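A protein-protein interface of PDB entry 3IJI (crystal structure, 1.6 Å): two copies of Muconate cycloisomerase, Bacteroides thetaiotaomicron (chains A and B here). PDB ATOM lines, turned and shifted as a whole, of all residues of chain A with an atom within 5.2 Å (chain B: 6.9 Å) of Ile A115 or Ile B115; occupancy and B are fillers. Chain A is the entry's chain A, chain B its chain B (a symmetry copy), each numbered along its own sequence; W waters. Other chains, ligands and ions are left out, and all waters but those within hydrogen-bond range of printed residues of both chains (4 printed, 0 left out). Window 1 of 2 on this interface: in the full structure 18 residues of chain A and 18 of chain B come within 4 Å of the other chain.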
ATOM      1  N   GLY A 105      27.045 -25.426   0.285  1.00  0.00           N
ATOM      2  CA  GLY A 105      25.638 -25.314  -0.064  1.00  0.00           C
ATOM      3  C   GLY A 105      24.957 -26.667   0.024  1.00  0.00           C
ATOM      4  O   GLY A 105      23.809 -26.777   0.457  1.00  0.00           O
ATOM      5  N   LEU A 108      24.402 -27.566   3.611  1.00  0.00           N
ATOM      6  CA  LEU A 108      23.308 -26.779   4.174  1.00  0.00           C
ATOM      7  C   LEU A 108      21.981 -27.139   3.525  1.00  0.00           C
ATOM      8  O   LEU A 108      20.918 -26.897   4.093  1.00  0.00           O
ATOM      9  CB  LEU A 108      23.558 -25.286   3.972  1.00  0.00           C
ATOM     10  CG  LEU A 108      24.486 -24.572   4.946  1.00  0.00           C
ATOM     11  CD1 LEU A 108      24.699 -23.143   4.475  1.00  0.00           C
ATOM     12  CD2 LEU A 108      23.870 -24.594   6.349  1.00  0.00           C
ATOM     13  N   ALA A 110      20.958 -25.931   0.486  1.00  0.00           N
ATOM     14  CA  ALA A 110      20.393 -24.759  -0.167  1.00  0.00           C
ATOM     15  C   ALA A 110      21.322 -24.164  -1.216  1.00  0.00           C
ATOM     16  O   ALA A 110      22.543 -24.265  -1.107  1.00  0.00           O
ATOM     17  CB  ALA A 110      20.057 -23.695   0.877  1.00  0.00           C
ATOM     18  N   PRO A 111      20.746 -23.554  -2.264  1.00  0.00           N
ATOM     19  CA  PRO A 111      21.559 -22.936  -3.316  1.00  0.00           C
ATOM     20  C   PRO A 111      22.057 -21.589  -2.793  1.00  0.00           C
ATOM     21  O   PRO A 111      21.435 -20.993  -1.909  1.00  0.00           O
ATOM     22  CB  PRO A 111      20.578 -22.802  -4.478  1.00  0.00           C
ATOM     23  CG  PRO A 111      19.268 -22.610  -3.796  1.00  0.00           C
ATOM     24  CD  PRO A 111      19.319 -23.575  -2.636  1.00  0.00           C
ATOM     25  N   TRP A 112      23.171 -21.097  -3.320  1.00  0.00           N
ATOM     26  CA  TRP A 112      23.679 -19.834  -2.819  1.00  0.00           C
ATOM     27  C   TRP A 112      22.815 -18.602  -3.039  1.00  0.00           C
ATOM     28  O   TRP A 112      22.860 -17.680  -2.234  1.00  0.00           O
ATOM     29  CB  TRP A 112      25.107 -19.601  -3.312  1.00  0.00           C
ATOM     30  CG  TRP A 112      26.064 -20.340  -2.440  1.00  0.00           C
ATOM     31  CD1 TRP A 112      26.488 -21.634  -2.589  1.00  0.00           C
ATOM     32  CD2 TRP A 112      26.596 -19.885  -1.193  1.00  0.00           C
ATOM     33  NE1 TRP A 112      27.243 -22.013  -1.503  1.00  0.00           N
ATOM     34  CE2 TRP A 112      27.325 -20.960  -0.631  1.00  0.00           C
ATOM     35  CE3 TRP A 112      26.524 -18.675  -0.489  1.00  0.00           C
ATOM     36  CZ2 TRP A 112      27.979 -20.859   0.602  1.00  0.00           C
ATOM     37  CZ3 TRP A 112      27.173 -18.576   0.737  1.00  0.00           C
ATOM     38  CH2 TRP A 112      27.891 -19.665   1.269  1.00  0.00           C
ATOM     39  N   TYR A 113      22.012 -18.570  -4.097  1.00  0.00           N
ATOM     40  CA  TYR A 113      21.168 -17.397  -4.291  1.00  0.00           C
ATOM     41  C   TYR A 113      20.221 -17.289  -3.091  1.00  0.00           C
ATOM     42  O   TYR A 113      19.873 -16.193  -2.659  1.00  0.00           O
ATOM     43  CB  TYR A 113      20.381 -17.491  -5.617  1.00  0.00           C
ATOM     44  CG  TYR A 113      19.180 -18.411  -5.602  1.00  0.00           C
ATOM     45  CD1 TYR A 113      17.994 -18.026  -4.977  1.00  0.00           C
ATOM     46  CD2 TYR A 113      19.231 -19.673  -6.201  1.00  0.00           C
ATOM     47  CE1 TYR A 113      16.889 -18.873  -4.940  1.00  0.00           C
ATOM     48  CE2 TYR A 113      18.125 -20.528  -6.170  1.00  0.00           C
ATOM     49  CZ  TYR A 113      16.961 -20.118  -5.534  1.00  0.00           C
ATOM     50  OH  TYR A 113      15.868 -20.959  -5.468  1.00  0.00           O
ATOM     51  N   LYS A 114      19.835 -18.435  -2.539  1.00  0.00           N
ATOM     52  CA  LYS A 114      18.927 -18.472  -1.397  1.00  0.00           C
ATOM     53  C   LYS A 114      19.669 -18.113  -0.113  1.00  0.00           C
ATOM     54  O   LYS A 114      19.157 -17.369   0.727  1.00  0.00           O
ATOM     55  CB  LYS A 114      18.298 -19.865  -1.289  1.00  0.00           C
ATOM     56  CG  LYS A 114      17.162 -19.987  -0.288  1.00  0.00           C
ATOM     57  CD  LYS A 114      16.464 -21.338  -0.455  1.00  0.00           C
ATOM     58  CE  LYS A 114      15.247 -21.467   0.445  1.00  0.00           C
ATOM     59  NZ  LYS A 114      14.590 -22.800   0.290  1.00  0.00           N
ATOM     60  N   ILE A 115      20.879 -18.644   0.037  1.00  0.00           N
ATOM     61  CA  ILE A 115      21.697 -18.362   1.210  1.00  0.00           C
ATOM     62  C   ILE A 115      22.006 -16.868   1.274  1.00  0.00           C
ATOM     63  O   ILE A 115      22.030 -16.278   2.358  1.00  0.00           O
ATOM     64  CB  ILE A 115      23.018 -19.170   1.169  1.00  0.00           C
ATOM     65  CG1 ILE A 115      22.695 -20.666   1.249  1.00  0.00           C
ATOM     66  CG2 ILE A 115      23.933 -18.757   2.327  1.00  0.00           C
ATOM     67  CD1 ILE A 115      23.883 -21.571   1.020  1.00  0.00           C
ATOM     68  N   TRP A 116      22.232 -16.257   0.112  1.00  0.00           N
ATOM     69  CA  TRP A 116      22.526 -14.829   0.036  1.00  0.00           C
ATOM     70  C   TRP A 116      21.271 -13.964   0.165  1.00  0.00           C
ATOM     71  O   TRP A 116      21.369 -12.739   0.230  1.00  0.00           O
ATOM     72  CB  TRP A 116      23.240 -14.486  -1.279  1.00  0.00           C
ATOM     73  CG  TRP A 116      24.693 -14.886  -1.316  1.00  0.00           C
ATOM     74  CD1 TRP A 116      25.584 -14.842  -0.280  1.00  0.00           C
ATOM     75  CD2 TRP A 116      25.443 -15.288  -2.471  1.00  0.00           C
ATOM     76  NE1 TRP A 116      26.844 -15.185  -0.719  1.00  0.00           N
ATOM     77  CE2 TRP A 116      26.786 -15.462  -2.060  1.00  0.00           C
ATOM     78  CE3 TRP A 116      25.113 -15.514  -3.813  1.00  0.00           C
ATOM     79  CZ2 TRP A 116      27.799 -15.850  -2.945  1.00  0.00           C
ATOM     80  CZ3 TRP A 116      26.122 -15.901  -4.695  1.00  0.00           C
ATOM     81  CH2 TRP A 116      27.448 -16.063  -4.254  1.00  0.00           C
ATOM     82  N   GLY A 117      20.100 -14.599   0.181  1.00  0.00           N
ATOM     83  CA  GLY A 117      18.846 -13.868   0.344  1.00  0.00           C
ATOM     84  C   GLY A 117      18.266 -13.206  -0.894  1.00  0.00           C
ATOM     85  O   GLY A 117      17.501 -12.245  -0.786  1.00  0.00           O
ATOM     86  N   PHE B  73      13.274 -16.598   3.044  1.00  0.00           N
ATOM     87  CA  PHE B  73      14.643 -16.518   2.547  1.00  0.00           C
ATOM     88  C   PHE B  73      14.950 -15.321   1.654  1.00  0.00           C
ATOM     89  O   PHE B  73      16.115 -14.984   1.460  1.00  0.00           O
ATOM     90  CB  PHE B  73      15.001 -17.809   1.799  1.00  0.00           C
ATOM     91  CG  PHE B  73      15.339 -18.961   2.703  1.00  0.00           C
ATOM     92  CD1 PHE B  73      16.655 -19.193   3.092  1.00  0.00           C
ATOM     93  CD2 PHE B  73      14.343 -19.810   3.176  1.00  0.00           C
ATOM     94  CE1 PHE B  73      16.977 -20.255   3.937  1.00  0.00           C
ATOM     95  CE2 PHE B  73      14.655 -20.877   4.024  1.00  0.00           C
ATOM     96  CZ  PHE B  73      15.974 -21.098   4.405  1.00  0.00           C
ATOM     97  N   LEU B  75      15.436 -12.284   1.878  1.00  0.00           N
ATOM     98  CA  LEU B  75      15.756 -11.164   2.754  1.00  0.00           C
ATOM     99  C   LEU B  75      16.075  -9.860   2.031  1.00  0.00           C
ATOM    100  O   LEU B  75      15.775  -8.784   2.539  1.00  0.00           O
ATOM    101  CB  LEU B  75      16.908 -11.549   3.687  1.00  0.00           C
ATOM    102  CG  LEU B  75      16.586 -12.699   4.648  1.00  0.00           C
ATOM    103  CD1 LEU B  75      17.786 -12.965   5.552  1.00  0.00           C
ATOM    104  CD2 LEU B  75      15.354 -12.344   5.483  1.00  0.00           C
ATOM    105  N   HIS B 101      16.314 -13.090  10.476  1.00  0.00           N
ATOM    106  CA  HIS B 101      17.554 -13.857  10.422  1.00  0.00           C
ATOM    107  C   HIS B 101      17.475 -15.055  11.346  1.00  0.00           C
ATOM    108  O   HIS B 101      17.970 -16.131  11.014  1.00  0.00           O
ATOM    109  CB  HIS B 101      18.753 -12.982  10.785  1.00  0.00           C
ATOM    110  CG  HIS B 101      19.143 -12.039   9.693  1.00  0.00           C
ATOM    111  ND1 HIS B 101      20.109 -12.337   8.754  1.00  0.00           N
ATOM    112  CD2 HIS B 101      18.639 -10.833   9.344  1.00  0.00           C
ATOM    113  CE1 HIS B 101      20.180 -11.354   7.874  1.00  0.00           C
ATOM    114  NE2 HIS B 101      19.298 -10.429   8.209  1.00  0.00           N
ATOM    115  N   VAL B 104      15.269 -17.573   9.439  1.00  0.00           N
ATOM    116  CA  VAL B 104      15.980 -18.179   8.320  1.00  0.00           C
ATOM    117  C   VAL B 104      17.079 -19.142   8.773  1.00  0.00           C
ATOM    118  O   VAL B 104      17.238 -20.220   8.196  1.00  0.00           O
ATOM    119  CB  VAL B 104      16.568 -17.089   7.392  1.00  0.00           C
ATOM    120  CG1 VAL B 104      17.486 -17.722   6.346  1.00  0.00           C
ATOM    121  CG2 VAL B 104      15.433 -16.351   6.699  1.00  0.00           C
ATOM    122  N   GLY B 105      17.825 -18.764   9.808  1.00  0.00           N
ATOM    123  CA  GLY B 105      18.883 -19.624  10.308  1.00  0.00           C
ATOM    124  C   GLY B 105      18.297 -20.912  10.852  1.00  0.00           C
ATOM    125  O   GLY B 105      18.861 -21.991  10.679  1.00  0.00           O
ATOM    126  N   LYS B 106      17.153 -20.796  11.516  1.00  0.00           N
ATOM    127  CA  LYS B 106      16.481 -21.969  12.062  1.00  0.00           C
ATOM    128  C   LYS B 106      15.977 -22.859  10.928  1.00  0.00           C
ATOM    129  O   LYS B 106      16.040 -24.088  11.023  1.00  0.00           O
ATOM    130  CB  LYS B 106      15.329 -21.535  12.975  1.00  0.00           C
ATOM    131  CG  LYS B 106      15.805 -21.033  14.332  1.00  0.00           C
ATOM    132  CD  LYS B 106      14.693 -20.352  15.119  1.00  0.00           C
ATOM    133  CE  LYS B 106      15.120 -20.062  16.547  1.00  0.00           C
ATOM    134  NZ  LYS B 106      15.438 -21.307  17.286  1.00  0.00           N
ATOM    135  N   LEU B 108      17.334 -23.137   8.042  1.00  0.00           N
ATOM    136  CA  LEU B 108      18.530 -23.731   7.440  1.00  0.00           C
ATOM    137  C   LEU B 108      19.269 -24.645   8.407  1.00  0.00           C
ATOM    138  O   LEU B 108      20.117 -25.435   7.993  1.00  0.00           O
ATOM    139  CB  LEU B 108      19.502 -22.646   6.985  1.00  0.00           C
ATOM    140  CG  LEU B 108      19.258 -21.958   5.650  1.00  0.00           C
ATOM    141  CD1 LEU B 108      20.249 -20.814   5.496  1.00  0.00           C
ATOM    142  CD2 LEU B 108      19.410 -22.971   4.516  1.00  0.00           C
ATOM    143  N   GLY B 109      18.964 -24.525   9.694  1.00  0.00           N
ATOM    144  CA  GLY B 109      19.629 -25.344  10.690  1.00  0.00           C
ATOM    145  C   GLY B 109      21.071 -24.940  10.949  1.00  0.00           C
ATOM    146  O   GLY B 109      21.934 -25.794  11.172  1.00  0.00           O
ATOM    147  N   ALA B 110      21.347 -23.640  10.920  1.00  0.00           N
ATOM    148  CA  ALA B 110      22.702 -23.162  11.157  1.00  0.00           C
ATOM    149  C   ALA B 110      22.734 -21.749  11.729  1.00  0.00           C
ATOM    150  O   ALA B 110      21.826 -20.954  11.489  1.00  0.00           O
ATOM    151  CB  ALA B 110      23.506 -23.204   9.856  1.00  0.00           C
ATOM    152  N   PRO B 111      23.778 -21.431  12.512  1.00  0.00           N
ATOM    153  CA  PRO B 111      23.940 -20.102  13.116  1.00  0.00           C
ATOM    154  C   PRO B 111      24.460 -19.178  12.023  1.00  0.00           C
ATOM    155  O   PRO B 111      25.122 -19.633  11.089  1.00  0.00           O
ATOM    156  CB  PRO B 111      25.008 -20.321  14.194  1.00  0.00           C
ATOM    157  CG  PRO B 111      25.065 -21.807  14.385  1.00  0.00           C
ATOM    158  CD  PRO B 111      24.797 -22.361  13.021  1.00  0.00           C
ATOM    159  N   TRP B 112      24.199 -17.883  12.132  1.00  0.00           N
ATOM    160  CA  TRP B 112      24.687 -16.985  11.097  1.00  0.00           C
ATOM    161  C   TRP B 112      26.204 -16.867  11.005  1.00  0.00           C
ATOM    162  O   TRP B 112      26.730 -16.622   9.925  1.00  0.00           O
ATOM    163  CB  TRP B 112      24.017 -15.609  11.215  1.00  0.00           C
ATOM    164  CG  TRP B 112      22.687 -15.640  10.539  1.00  0.00           C
ATOM    165  CD1 TRP B 112      21.483 -15.987  11.097  1.00  0.00           C
ATOM    166  CD2 TRP B 112      22.445 -15.484   9.137  1.00  0.00           C
ATOM    167  NE1 TRP B 112      20.516 -16.065  10.125  1.00  0.00           N
ATOM    168  CE2 TRP B 112      21.079 -15.760   8.912  1.00  0.00           C
ATOM    169  CE3 TRP B 112      23.255 -15.143   8.047  1.00  0.00           C
ATOM    170  CZ2 TRP B 112      20.502 -15.703   7.638  1.00  0.00           C
ATOM    171  CZ3 TRP B 112      22.684 -15.087   6.780  1.00  0.00           C
ATOM    172  CH2 TRP B 112      21.316 -15.367   6.589  1.00  0.00           C
ATOM    173  N   TYR B 113      26.928 -17.059  12.106  1.00  0.00           N
ATOM    174  CA  TYR B 113      28.381 -16.967  12.002  1.00  0.00           C
ATOM    175  C   TYR B 113      28.856 -18.049  11.026  1.00  0.00           C
ATOM    176  O   TYR B 113      29.799 -17.840  10.259  1.00  0.00           O
ATOM    177  CB  TYR B 113      29.057 -17.129  13.381  1.00  0.00           C
ATOM    178  CG  TYR B 113      29.155 -18.548  13.910  1.00  0.00           C
ATOM    179  CD1 TYR B 113      30.095 -19.443  13.394  1.00  0.00           C
ATOM    180  CD2 TYR B 113      28.300 -18.998  14.915  1.00  0.00           C
ATOM    181  CE1 TYR B 113      30.176 -20.755  13.863  1.00  0.00           C
ATOM    182  CE2 TYR B 113      28.375 -20.310  15.392  1.00  0.00           C
ATOM    183  CZ  TYR B 113      29.315 -21.180  14.858  1.00  0.00           C
ATOM    184  OH  TYR B 113      29.377 -22.487  15.303  1.00  0.00           O
ATOM    185  N   LYS B 114      28.168 -19.187  11.033  1.00  0.00           N
ATOM    186  CA  LYS B 114      28.522 -20.306  10.160  1.00  0.00           C
ATOM    187  C   LYS B 114      28.087 -20.050   8.721  1.00  0.00           C
ATOM    188  O   LYS B 114      28.822 -20.347   7.776  1.00  0.00           O
ATOM    189  CB  LYS B 114      27.881 -21.592  10.689  1.00  0.00           C
ATOM    190  CG  LYS B 114      28.242 -22.849   9.907  1.00  0.00           C
ATOM    191  CD  LYS B 114      27.795 -24.111  10.642  1.00  0.00           C
ATOM    192  CE  LYS B 114      28.543 -24.275  11.954  1.00  0.00           C
ATOM    193  NZ  LYS B 114      28.237 -25.571  12.625  1.00  0.00           N
ATOM    194  N   ILE B 115      26.888 -19.504   8.557  1.00  0.00           N
ATOM    195  CA  ILE B 115      26.373 -19.190   7.231  1.00  0.00           C
ATOM    196  C   ILE B 115      27.295 -18.158   6.582  1.00  0.00           C
ATOM    197  O   ILE B 115      27.574 -18.228   5.381  1.00  0.00           O
ATOM    198  CB  ILE B 115      24.934 -18.626   7.318  1.00  0.00           C
ATOM    199  CG1 ILE B 115      23.995 -19.710   7.863  1.00  0.00           C
ATOM    200  CG2 ILE B 115      24.472 -18.144   5.947  1.00  0.00           C
ATOM    201  CD1 ILE B 115      22.619 -19.206   8.267  1.00  0.00           C
ATOM    202  N   TRP B 116      27.772 -17.204   7.382  1.00  0.00           N
ATOM    203  CA  TRP B 116      28.667 -16.166   6.875  1.00  0.00           C
ATOM    204  C   TRP B 116      30.097 -16.669   6.673  1.00  0.00           C
ATOM    205  O   TRP B 116      30.947 -15.938   6.166  1.00  0.00           O
ATOM    206  CB  TRP B 116      28.679 -14.948   7.810  1.00  0.00           C
ATOM    207  CG  TRP B 116      27.448 -14.082   7.722  1.00  0.00           C
ATOM    208  CD1 TRP B 116      26.704 -13.812   6.604  1.00  0.00           C
ATOM    209  CD2 TRP B 116      26.881 -13.295   8.777  1.00  0.00           C
ATOM    210  NE1 TRP B 116      25.712 -12.903   6.901  1.00  0.00           N
ATOM    211  CE2 TRP B 116      25.800 -12.569   8.227  1.00  0.00           C
ATOM    212  CE3 TRP B 116      27.185 -13.132  10.135  1.00  0.00           C
ATOM    213  CZ2 TRP B 116      25.021 -11.689   8.989  1.00  0.00           C
ATOM    214  CZ3 TRP B 116      26.410 -12.254  10.897  1.00  0.00           C
ATOM    215  CH2 TRP B 116      25.340 -11.545  10.320  1.00  0.00           C
ATOM    216  N   GLY B 117      30.358 -17.908   7.082  1.00  0.00           N
ATOM    217  CA  GLY B 117      31.675 -18.504   6.900  1.00  0.00           C
ATOM    218  C   GLY B 117      32.759 -18.092   7.877  1.00  0.00           C
ATOM    219  O   GLY B 117      33.951 -18.165   7.560  1.00  0.00           O
ATOM    220  N   LEU B 118      32.355 -17.686   9.076  1.00  0.00           N
ATOM    221  CA  LEU B 118      33.302 -17.241  10.091  1.00  0.00           C
ATOM    222  C   LEU B 118      33.698 -18.334  11.077  1.00  0.00           C
ATOM    223  O   LEU B 118      32.982 -19.314  11.260  1.00  0.00           O
ATOM    224  CB  LEU B 118      32.707 -16.063  10.865  1.00  0.00           C
ATOM    225  CG  LEU B 118      32.200 -14.931   9.970  1.00  0.00           C
ATOM    226  CD1 LEU B 118      31.550 -13.856  10.831  1.00  0.00           C
ATOM    227  CD2 LEU B 118      33.355 -14.345   9.158  1.00  0.00           C
ATOM    228  N   ARG B 261      21.664  -7.808   8.345  1.00  0.00           N
ATOM    229  CA  ARG B 261      22.011  -7.783   6.930  1.00  0.00           C
ATOM    230  C   ARG B 261      22.821  -6.548   6.562  1.00  0.00           C
ATOM    231  O   ARG B 261      23.843  -6.649   5.882  1.00  0.00           O
ATOM    232  CB  ARG B 261      20.754  -7.884   6.057  1.00  0.00           C
ATOM    233  CG  ARG B 261      21.068  -8.117   4.574  1.00  0.00           C
ATOM    234  CD  ARG B 261      19.807  -8.414   3.776  1.00  0.00           C
ATOM    235  NE  ARG B 261      20.087  -8.656   2.358  1.00  0.00           N
ATOM    236  CZ  ARG B 261      20.458  -9.828   1.849  1.00  0.00           C
ATOM    237  NH1 ARG B 261      20.599 -10.889   2.632  1.00  0.00           N
ATOM    238  NH2 ARG B 261      20.679  -9.941   0.543  1.00  0.00           N
ATOM    239  N   GLN B 294      26.992 -12.701  16.195  1.00  0.00           N
ATOM    240  CA  GLN B 294      27.171 -13.605  15.059  1.00  0.00           C
ATOM    241  C   GLN B 294      28.255 -13.147  14.078  1.00  0.00           C
ATOM    242  O   GLN B 294      28.845 -13.975  13.383  1.00  0.00           O
ATOM    243  CB  GLN B 294      25.842 -13.822  14.324  1.00  0.00           C
ATOM    244  CG  GLN B 294      24.772 -14.581  15.136  1.00  0.00           C
ATOM    245  CD  GLN B 294      25.166 -16.014  15.484  1.00  0.00           C
ATOM    246  OE1 GLN B 294      25.800 -16.709  14.692  1.00  0.00           O
ATOM    247  NE2 GLN B 294      24.766 -16.467  16.671  1.00  0.00           N
ATOM    248  N   GLY B 332      20.197 -19.829  13.753  1.00  0.00           N
ATOM    249  CA  GLY B 332      19.668 -18.477  13.777  1.00  0.00           C
ATOM    250  C   GLY B 332      20.606 -17.531  14.499  1.00  0.00           C
ATOM    251  O   GLY B 332      21.805 -17.511  14.219  1.00  0.00           O
HETATM  252  O   HOH W   1      18.501 -15.756   3.099  1.00  0.00           O
HETATM  253  O   HOH W   2      20.215 -27.507   6.469  1.00  0.00           O
HETATM  254  O   HOH W   3      23.750 -11.505   1.066  1.00  0.00           O
HETATM  255  O   HOH W   4      20.649 -13.924   3.397  1.00  0.00           O
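The backbone carbonyl oxygen (O) of Trp A116 sits at hydrogen-bond distance from the guanidinium group (NH2) of Arg B261, 2.9 Å away.
The backbone carbonyl oxygen (O) of Gly A117 sits at hydrogen-bond distance from the backbone NH (N) of Leu B75 (3.4 Å).
The backbone carbonyl oxygen of Gly A105 lies within hydrogen-bond range of the backbone NH of Ala A110 (3.0 Å).
O of Gly B105 is in hydrogen-bond range of N of Ala B110, 3.0 Å away.
The backbone carbonyl oxygen (O) of Ala B110 is in hydrogen-bond range of the backbone NH (N) of Gly B332.
CB of Ala B110 touches CD2 of Leu A108 (3.8 Å).
Leu B108 touches Ala A110 (CD2 to CB, 3.8 Å).
Lys A114 touches Phe B73 (CE to CD2, 3.3 Å).
Ile A115 touches Ile B115 (CG2 to CG2, 3.7 Å).
Gly A117 touches Phe B73.
Printed residues of chain B within 4 Å of Ala A110: Leu B108 (3.8 Å).
Pro A111 touches none of the printed residues of chain B.
Of chain B, only Ile B115 (3.7 Å) comes within 4 Å of Ile A115.
Of the printed residues of chain B, Gly A117 touches Phe B73 (3.2 Å) and Leu B75 (3.4 Å).
Of the printed residues of chain A, Leu B75 touches Gly A117 (3.4 Å).
Gly B109 touches none of the printed residues of chain A.
Ile B115 touches just one residue of chain A: Ile A115 (3.7 Å).
Of the printed residues of chain A, Arg B261 touches Trp A116.
The nearest residue of chain A that does not touch Ile B115 is Trp A112 (4.4 Å).
The nearest printed residue of chain B that does not touch Ala A110 is Phe B73 (5.5 Å).
Hydrophobic or aromatic side chains of chain B within 4 Å of the printed part of chain A: Phe B73, Leu B108, Ala B110 and Ile B115.
Among the printed residues, 7 pairs touch across the chains.
Leu A108 touches Ala B110, and with the chains exchanged Ala A110 touches Leu B108.
Ile B115 touches its own counterpart, Ile A115.
Positions printed for both chains: 105, 108, 110, 111, 112, 113, 114, 115, 116 and 117.
Water W2 bridges the backbone carbonyl oxygen (O) of Leu A108 (2.6 Å) and the backbone carbonyl oxygen (O) of Leu B108 (2.6 Å).
Water W3 bridges the backbone carbonyl oxygen (O) of Trp A116 (2.8 Å) and the guanidinium group (NH2) of Arg B261 (3.5 Å).
Water W4 lies within hydrogen-bond range of the backbone carbonyl oxygen (O) of Ile A115 (2.9 Å), the guanidinium group (NH1) of Arg B261 (3.1 Å), the backbone NH (N) of Gly A117 (3.3 Å) and the backbone carbonyl oxygen (O) of Trp A116 (3.5 Å).
Water W1 lies within hydrogen-bond range of the backbone carbonyl oxygen (O) of Lys A114 (2.9 Å) and the backbone carbonyl oxygen (O) of Phe B73 (3.0 Å).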
